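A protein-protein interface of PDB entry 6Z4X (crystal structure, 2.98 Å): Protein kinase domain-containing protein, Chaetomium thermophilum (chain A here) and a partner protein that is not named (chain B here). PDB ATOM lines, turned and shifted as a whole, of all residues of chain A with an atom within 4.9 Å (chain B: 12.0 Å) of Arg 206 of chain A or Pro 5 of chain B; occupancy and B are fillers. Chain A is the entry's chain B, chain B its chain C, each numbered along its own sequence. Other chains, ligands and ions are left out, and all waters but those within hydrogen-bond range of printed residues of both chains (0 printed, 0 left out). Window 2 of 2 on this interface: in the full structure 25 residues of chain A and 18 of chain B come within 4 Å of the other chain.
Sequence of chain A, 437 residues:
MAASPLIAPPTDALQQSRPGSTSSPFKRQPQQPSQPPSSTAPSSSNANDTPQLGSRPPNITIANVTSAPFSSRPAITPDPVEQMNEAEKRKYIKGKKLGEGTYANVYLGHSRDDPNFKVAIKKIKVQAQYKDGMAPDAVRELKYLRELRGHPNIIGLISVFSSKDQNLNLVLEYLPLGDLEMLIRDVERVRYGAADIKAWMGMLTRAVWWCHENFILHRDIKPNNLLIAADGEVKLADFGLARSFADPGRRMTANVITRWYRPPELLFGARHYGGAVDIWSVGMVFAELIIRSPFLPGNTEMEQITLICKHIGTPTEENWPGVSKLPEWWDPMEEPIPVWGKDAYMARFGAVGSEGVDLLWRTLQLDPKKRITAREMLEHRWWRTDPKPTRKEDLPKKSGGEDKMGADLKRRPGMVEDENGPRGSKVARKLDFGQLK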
ATOM      1  N   HIS A 151      -9.560  -5.183   7.348  1.00  0.00           N
ATOM      2  CA  HIS A 151      -9.362  -4.904   5.935  1.00  0.00           C
ATOM      3  C   HIS A 151      -7.890  -5.043   5.570  1.00  0.00           C
ATOM      4  O   HIS A 151      -7.014  -4.669   6.361  1.00  0.00           O
ATOM      5  CB  HIS A 151      -9.845  -3.495   5.592  1.00  0.00           C
ATOM      6  CG  HIS A 151     -10.008  -3.249   4.125  1.00  0.00           C
ATOM      7  ND1 HIS A 151      -9.022  -2.676   3.351  1.00  0.00           N
ATOM      8  CD2 HIS A 151     -11.040  -3.506   3.288  1.00  0.00           C
ATOM      9  CE1 HIS A 151      -9.443  -2.584   2.101  1.00  0.00           C
ATOM     10  NE2 HIS A 151     -10.664  -3.082   2.036  1.00  0.00           N
ATOM     11  N   ASN A 153      -6.029  -3.393   3.633  1.00  0.00           N
ATOM     12  CA  ASN A 153      -5.336  -2.146   3.338  1.00  0.00           C
ATOM     13  C   ASN A 153      -5.393  -1.147   4.491  1.00  0.00           C
ATOM     14  O   ASN A 153      -5.175   0.050   4.281  1.00  0.00           O
ATOM     15  CB  ASN A 153      -5.894  -1.531   2.055  1.00  0.00           C
ATOM     16  CG  ASN A 153      -5.710  -2.438   0.849  1.00  0.00           C
ATOM     17  OD1 ASN A 153      -6.678  -2.922   0.264  1.00  0.00           O
ATOM     18  ND2 ASN A 153      -4.458  -2.669   0.471  1.00  0.00           N
ATOM     19  N   MET A 201      -2.607   3.048  -6.148  1.00  0.00           N
ATOM     20  CA  MET A 201      -3.828   3.831  -6.025  1.00  0.00           C
ATOM     21  C   MET A 201      -5.020   2.940  -5.719  1.00  0.00           C
ATOM     22  O   MET A 201      -5.934   3.345  -4.996  1.00  0.00           O
ATOM     23  CB  MET A 201      -4.071   4.639  -7.297  1.00  0.00           C
ATOM     24  CG  MET A 201      -3.170   5.852  -7.431  1.00  0.00           C
ATOM     25  SD  MET A 201      -3.423   7.024  -6.086  1.00  0.00           S
ATOM     26  CE  MET A 201      -5.142   7.459  -6.336  1.00  0.00           C
ATOM     27  N   GLY A 202      -5.038   1.725  -6.267  1.00  0.00           N
ATOM     28  CA  GLY A 202      -6.093   0.792  -5.906  1.00  0.00           C
ATOM     29  C   GLY A 202      -6.078   0.473  -4.425  1.00  0.00           C
ATOM     30  O   GLY A 202      -7.117   0.489  -3.760  1.00  0.00           O
ATOM     31  N   MET A 203      -4.890   0.197  -3.885  1.00  0.00           N
ATOM     32  CA  MET A 203      -4.770  -0.066  -2.453  1.00  0.00           C
ATOM     33  C   MET A 203      -5.266   1.122  -1.632  1.00  0.00           C
ATOM     34  O   MET A 203      -6.066   0.964  -0.700  1.00  0.00           O
ATOM     35  CB  MET A 203      -3.320  -0.387  -2.098  1.00  0.00           C
ATOM     36  CG  MET A 203      -2.809  -1.679  -2.687  1.00  0.00           C
ATOM     37  SD  MET A 203      -1.042  -1.877  -2.450  1.00  0.00           S
ATOM     38  CE  MET A 203      -0.801  -3.512  -3.143  1.00  0.00           C
ATOM     39  N   LEU A 204      -4.791   2.323  -1.967  1.00  0.00           N
ATOM     40  CA  LEU A 204      -5.172   3.513  -1.209  1.00  0.00           C
ATOM     41  C   LEU A 204      -6.675   3.763  -1.287  1.00  0.00           C
ATOM     42  O   LEU A 204      -7.322   4.071  -0.277  1.00  0.00           O
ATOM     43  CB  LEU A 204      -4.394   4.730  -1.717  1.00  0.00           C
ATOM     44  CG  LEU A 204      -4.841   6.081  -1.152  1.00  0.00           C
ATOM     45  CD1 LEU A 204      -4.818   6.067   0.367  1.00  0.00           C
ATOM     46  CD2 LEU A 204      -3.968   7.206  -1.690  1.00  0.00           C
ATOM     47  N   THR A 205      -7.244   3.652  -2.490  1.00  0.00           N
ATOM     48  CA  THR A 205      -8.668   3.892  -2.663  1.00  0.00           C
ATOM     49  C   THR A 205      -9.490   2.861  -1.907  1.00  0.00           C
ATOM     50  O   THR A 205     -10.529   3.194  -1.331  1.00  0.00           O
ATOM     51  CB  THR A 205      -9.027   3.887  -4.147  1.00  0.00           C
ATOM     52  OG1 THR A 205      -8.315   4.938  -4.811  1.00  0.00           O
ATOM     53  CG2 THR A 205     -10.514   4.108  -4.328  1.00  0.00           C
ATOM     54  N   ARG A 206      -9.041   1.603  -1.888  1.00  0.00           N
ATOM     55  CA  ARG A 206      -9.770   0.593  -1.129  1.00  0.00           C
ATOM     56  C   ARG A 206      -9.695   0.874   0.366  1.00  0.00           C
ATOM     57  O   ARG A 206     -10.687   0.703   1.086  1.00  0.00           O
ATOM     58  CB  ARG A 206      -9.245  -0.804  -1.465  1.00  0.00           C
ATOM     59  CG  ARG A 206      -9.691  -1.267  -2.837  1.00  0.00           C
ATOM     60  CD  ARG A 206      -9.206  -2.657  -3.208  1.00  0.00           C
ATOM     61  NE  ARG A 206      -9.823  -3.076  -4.465  1.00  0.00           N
ATOM     62  CZ  ARG A 206      -9.350  -2.769  -5.670  1.00  0.00           C
ATOM     63  NH1 ARG A 206      -8.244  -2.046  -5.782  1.00  0.00           N
ATOM     64  NH2 ARG A 206      -9.987  -3.181  -6.761  1.00  0.00           N
ATOM     65  N   ALA A 207      -8.539   1.338   0.844  1.00  0.00           N
ATOM     66  CA  ALA A 207      -8.418   1.691   2.255  1.00  0.00           C
ATOM     67  C   ALA A 207      -9.367   2.829   2.619  1.00  0.00           C
ATOM     68  O   ALA A 207     -10.076   2.767   3.632  1.00  0.00           O
ATOM     69  CB  ALA A 207      -6.972   2.066   2.579  1.00  0.00           C
ATOM     70  N   VAL A 208      -9.393   3.883   1.801  1.00  0.00           N
ATOM     71  CA  VAL A 208     -10.267   5.016   2.099  1.00  0.00           C
ATOM     72  C   VAL A 208     -11.733   4.616   1.967  1.00  0.00           C
ATOM     73  O   VAL A 208     -12.591   5.099   2.718  1.00  0.00           O
ATOM     74  CB  VAL A 208      -9.924   6.219   1.203  1.00  0.00           C
ATOM     75  CG1 VAL A 208     -10.915   7.344   1.443  1.00  0.00           C
ATOM     76  CG2 VAL A 208      -8.508   6.693   1.486  1.00  0.00           C
ATOM     77  N   TRP A 209     -12.051   3.748   1.002  1.00  0.00           N
ATOM     78  CA  TRP A 209     -13.423   3.275   0.871  1.00  0.00           C
ATOM     79  C   TRP A 209     -13.847   2.498   2.104  1.00  0.00           C
ATOM     80  O   TRP A 209     -14.981   2.635   2.571  1.00  0.00           O
ATOM     81  CB  TRP A 209     -13.583   2.408  -0.378  1.00  0.00           C
ATOM     82  CG  TRP A 209     -14.881   1.652  -0.375  1.00  0.00           C
ATOM     83  CD1 TRP A 209     -16.096   2.113  -0.791  1.00  0.00           C
ATOM     84  CD2 TRP A 209     -15.097   0.313   0.088  1.00  0.00           C
ATOM     85  NE1 TRP A 209     -17.053   1.141  -0.623  1.00  0.00           N
ATOM     86  CE2 TRP A 209     -16.465   0.027  -0.085  1.00  0.00           C
ATOM     87  CE3 TRP A 209     -14.266  -0.672   0.630  1.00  0.00           C
ATOM     88  CZ2 TRP A 209     -17.022  -1.202   0.263  1.00  0.00           C
ATOM     89  CZ3 TRP A 209     -14.821  -1.892   0.974  1.00  0.00           C
ATOM     90  CH2 TRP A 209     -16.186  -2.146   0.789  1.00  0.00           C
ATOM     91  N   TRP A 210     -12.955   1.661   2.638  1.00  0.00           N
ATOM     92  CA  TRP A 210     -13.280   0.932   3.859  1.00  0.00           C
ATOM     93  C   TRP A 210     -13.443   1.888   5.033  1.00  0.00           C
ATOM     94  O   TRP A 210     -14.322   1.693   5.884  1.00  0.00           O
ATOM     95  CB  TRP A 210     -12.210  -0.120   4.142  1.00  0.00           C
ATOM     96  CG  TRP A 210     -12.511  -0.971   5.333  1.00  0.00           C
ATOM     97  CD1 TRP A 210     -11.756  -1.095   6.461  1.00  0.00           C
ATOM     98  CD2 TRP A 210     -13.663  -1.805   5.528  1.00  0.00           C
ATOM     99  NE1 TRP A 210     -12.354  -1.966   7.340  1.00  0.00           N
ATOM    100  CE2 TRP A 210     -13.528  -2.414   6.792  1.00  0.00           C
ATOM    101  CE3 TRP A 210     -14.793  -2.098   4.754  1.00  0.00           C
ATOM    102  CZ2 TRP A 210     -14.477  -3.299   7.300  1.00  0.00           C
ATOM    103  CZ3 TRP A 210     -15.735  -2.978   5.263  1.00  0.00           C
ATOM    104  CH2 TRP A 210     -15.571  -3.566   6.522  1.00  0.00           C
ATOM    105  N   LEU A 378     -13.774   3.424  -6.851  1.00  0.00           N
ATOM    106  CA  LEU A 378     -13.472   2.019  -7.094  1.00  0.00           C
ATOM    107  C   LEU A 378     -14.186   1.482  -8.326  1.00  0.00           C
ATOM    108  O   LEU A 378     -13.767   0.456  -8.874  1.00  0.00           O
ATOM    109  CB  LEU A 378     -13.838   1.166  -5.876  1.00  0.00           C
ATOM    110  CG  LEU A 378     -12.907   1.260  -4.666  1.00  0.00           C
ATOM    111  CD1 LEU A 378     -13.461   0.467  -3.493  1.00  0.00           C
ATOM    112  CD2 LEU A 378     -11.517   0.764  -5.040  1.00  0.00           C
ATOM    113  N   ASP B   4     -14.242  -8.500  -8.887  1.00  0.00           N
ATOM    114  CA  ASP B   4     -14.897  -7.780  -7.800  1.00  0.00           C
ATOM    115  C   ASP B   4     -14.061  -6.564  -7.402  1.00  0.00           C
ATOM    116  O   ASP B   4     -12.952  -6.707  -6.890  1.00  0.00           O
ATOM    117  CB  ASP B   4     -15.115  -8.708  -6.601  1.00  0.00           C
ATOM    118  CG  ASP B   4     -15.949  -8.069  -5.510  1.00  0.00           C
ATOM    119  OD1 ASP B   4     -17.164  -7.886  -5.727  1.00  0.00           O
ATOM    120  OD2 ASP B   4     -15.393  -7.761  -4.435  1.00  0.00           O
ATOM    121  N   PRO B   5     -14.599  -5.364  -7.637  1.00  0.00           N
ATOM    122  CA  PRO B   5     -13.805  -4.149  -7.398  1.00  0.00           C
ATOM    123  C   PRO B   5     -13.583  -3.834  -5.932  1.00  0.00           C
ATOM    124  O   PRO B   5     -12.606  -3.147  -5.610  1.00  0.00           O
ATOM    125  CB  PRO B   5     -14.631  -3.051  -8.082  1.00  0.00           C
ATOM    126  CG  PRO B   5     -16.033  -3.563  -8.034  1.00  0.00           C
ATOM    127  CD  PRO B   5     -15.938  -5.061  -8.172  1.00  0.00           C
ATOM    128  N   PHE B   6     -14.442  -4.310  -5.034  1.00  0.00           N
ATOM    129  CA  PHE B   6     -14.311  -4.034  -3.611  1.00  0.00           C
ATOM    130  C   PHE B   6     -13.485  -5.082  -2.873  1.00  0.00           C
ATOM    131  O   PHE B   6     -13.524  -5.127  -1.640  1.00  0.00           O
ATOM    132  CB  PHE B   6     -15.694  -3.911  -2.967  1.00  0.00           C
ATOM    133  CG  PHE B   6     -16.576  -2.881  -3.612  1.00  0.00           C
ATOM    134  CD1 PHE B   6     -16.393  -1.532  -3.351  1.00  0.00           C
ATOM    135  CD2 PHE B   6     -17.592  -3.260  -4.474  1.00  0.00           C
ATOM    136  CE1 PHE B   6     -17.202  -0.580  -3.943  1.00  0.00           C
ATOM    137  CE2 PHE B   6     -18.407  -2.311  -5.068  1.00  0.00           C
ATOM    138  CZ  PHE B   6     -18.211  -0.969  -4.801  1.00  0.00           C
ATOM    139  N   GLY B   7     -12.743  -5.918  -3.593  1.00  0.00           N
ATOM    140  CA  GLY B   7     -11.922  -6.929  -2.943  1.00  0.00           C
ATOM    141  C   GLY B   7     -12.706  -7.877  -2.063  1.00  0.00           C
ATOM    142  O   GLY B   7     -12.203  -8.312  -1.019  1.00  0.00           O
ATOM    143  N   GLY B   8     -13.931  -8.212  -2.464  1.00  0.00           N
ATOM    144  CA  GLY B   8     -14.759  -9.113  -1.686  1.00  0.00           C
ATOM    145  C   GLY B   8     -15.198  -8.579  -0.342  1.00  0.00           C
ATOM    146  O   GLY B   8     -15.629  -9.358   0.511  1.00  0.00           O
ATOM    147  N   MET B   9     -15.109  -7.268  -0.129  1.00  0.00           N
ATOM    148  CA  MET B   9     -15.505  -6.654   1.130  1.00  0.00           C
ATOM    149  C   MET B   9     -16.765  -5.809   1.007  1.00  0.00           C
ATOM    150  O   MET B   9     -17.168  -5.179   1.991  1.00  0.00           O
ATOM    151  CB  MET B   9     -14.367  -5.783   1.677  1.00  0.00           C
ATOM    152  CG  MET B   9     -13.043  -6.502   1.841  1.00  0.00           C
ATOM    153  SD  MET B   9     -13.024  -7.644   3.234  1.00  0.00           S
ATOM    154  CE  MET B   9     -11.457  -8.468   2.964  1.00  0.00           C
ATOM    155  N   GLU B  10     -17.396  -5.782  -0.165  1.00  0.00           N
ATOM    156  CA  GLU B  10     -18.536  -4.902  -0.377  1.00  0.00           C
ATOM    157  C   GLU B  10     -19.638  -5.192   0.633  1.00  0.00           C
ATOM    158  O   GLU B  10     -20.025  -6.345   0.838  1.00  0.00           O
ATOM    159  CB  GLU B  10     -19.067  -5.049  -1.802  1.00  0.00           C
ATOM    160  CG  GLU B  10     -20.247  -4.135  -2.105  1.00  0.00           C
ATOM    161  CD  GLU B  10     -20.700  -4.220  -3.546  1.00  0.00           C
ATOM    162  OE1 GLU B  10     -21.389  -3.287  -4.007  1.00  0.00           O
ATOM    163  OE2 GLU B  10     -20.365  -5.216  -4.220  1.00  0.00           O
ATOM    164  N   PHE B  11     -20.141  -4.134   1.264  1.00  0.00           N
ATOM    165  CA  PHE B  11     -21.227  -4.242   2.227  1.00  0.00           C
ATOM    166  C   PHE B  11     -22.558  -4.036   1.513  1.00  0.00           C
ATOM    167  O   PHE B  11     -22.815  -2.956   0.968  1.00  0.00           O
ATOM    168  CB  PHE B  11     -21.057  -3.221   3.351  1.00  0.00           C
ATOM    169  CG  PHE B  11     -22.259  -3.099   4.244  1.00  0.00           C
ATOM    170  CD1 PHE B  11     -22.569  -4.096   5.152  1.00  0.00           C
ATOM    171  CD2 PHE B  11     -23.080  -1.987   4.174  1.00  0.00           C
ATOM    172  CE1 PHE B  11     -23.674  -3.988   5.973  1.00  0.00           C
ATOM    173  CE2 PHE B  11     -24.187  -1.873   4.992  1.00  0.00           C
ATOM    174  CZ  PHE B  11     -24.485  -2.875   5.892  1.00  0.00           C
ATOM    175  N   VAL B  12     -23.391  -5.071   1.507  1.00  0.00           N
ATOM    176  CA  VAL B  12     -24.730  -4.991   0.929  1.00  0.00           C
ATOM    177  C   VAL B  12     -25.741  -5.371   2.006  1.00  0.00           C
ATOM    178  O   VAL B  12     -25.819  -6.546   2.395  1.00  0.00           O
ATOM    179  CB  VAL B  12     -24.864  -5.887  -0.311  1.00  0.00           C
ATOM    180  CG1 VAL B  12     -24.157  -5.252  -1.499  1.00  0.00           C
ATOM    181  CG2 VAL B  12     -24.302  -7.268  -0.032  1.00  0.00           C
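Of the 13 printed residues of chain A, 4 touch a printed residue of chain B. Printed residues of chain A that touch a printed residue of chain B: His 151, Arg 206, Trp 209 and Leu 378. Hydrophobic or aromatic side chains of chain A within 4 Å of the printed part of chain B: His 151, Trp 209 and Leu 378. Along chain A the printed residues that touch a printed residue of chain B span positions 151 to 378. Of the 9 printed residues of chain B, 4 touch a printed residue of chain A. Printed residues of chain B that touch a printed residue of chain A: Pro 5, Phe 6, Met 9 and Glu 10. Among the printed residues, 7 pairs touch across the chains.
NH2 of Arg 206 of chain A sits at hydrogen-bond distance from O of Pro 5 of chain B (2.9 Å).
Among the printed residues, merely in contact across the chains: Trp 209 of chain A with Met 9 of chain B (3.4 Å), Leu 378 of chain A with Phe 6 of chain B (3.6 Å), Trp 209 of chain A with Phe 6 of chain B (3.6 Å), Leu 378 of chain A with Pro 5 of chain B (3.7 Å), Trp 209 of chain A with Glu 10 of chain B (3.8 Å) and His 151 of chain A with Met 9 of chain B (3.9 Å).
A ring nitrogen (ND1) of His 151 of chain A lies within hydrogen-bond range of the backbone NH (N) of Asn 153 of chain A (3.1 Å). The guanidinium group (NH1) of Arg 206 of chain A lies close to the backbone carbonyl oxygen (O) of Gly 202 of chain A.
Of the printed residues of chain B, His 151 of chain A touches Met 9 (3.9 Å). No residue of chain B comes within 4 Å of Asn 153 of chain A. No residue of chain B comes within 4 Å of Gly 202 of chain A. No residue of chain B comes within 4 Å of Leu 204 of chain A. Of the printed residues of chain B, Arg 206 of chain A touches Pro 5. No residue of chain B comes within 4 Å of Val 208 of chain A. Leu 378 of chain A touches two residues of chain B. Of chain A, only Arg 206 (2.9 Å) and Leu 378 (3.7 Å) come within 4 Å of Pro 5 of chain B. Of the printed residues of chain A, Phe 6 of chain B touches Trp 209 and Leu 378. Of the printed residues of chain A, Met 9 of chain B touches His 151 and Trp 209. Of the printed residues of chain A, Glu 10 of chain B touches Trp 209. The nearest residue of chain B that does not touch Arg 206 of chain A is Gly 7 of chain B (4.2 Å). The nearest printed residue of chain A that does not touch Pro 5 of chain B is Gly 202 of chain A (6.8 Å).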
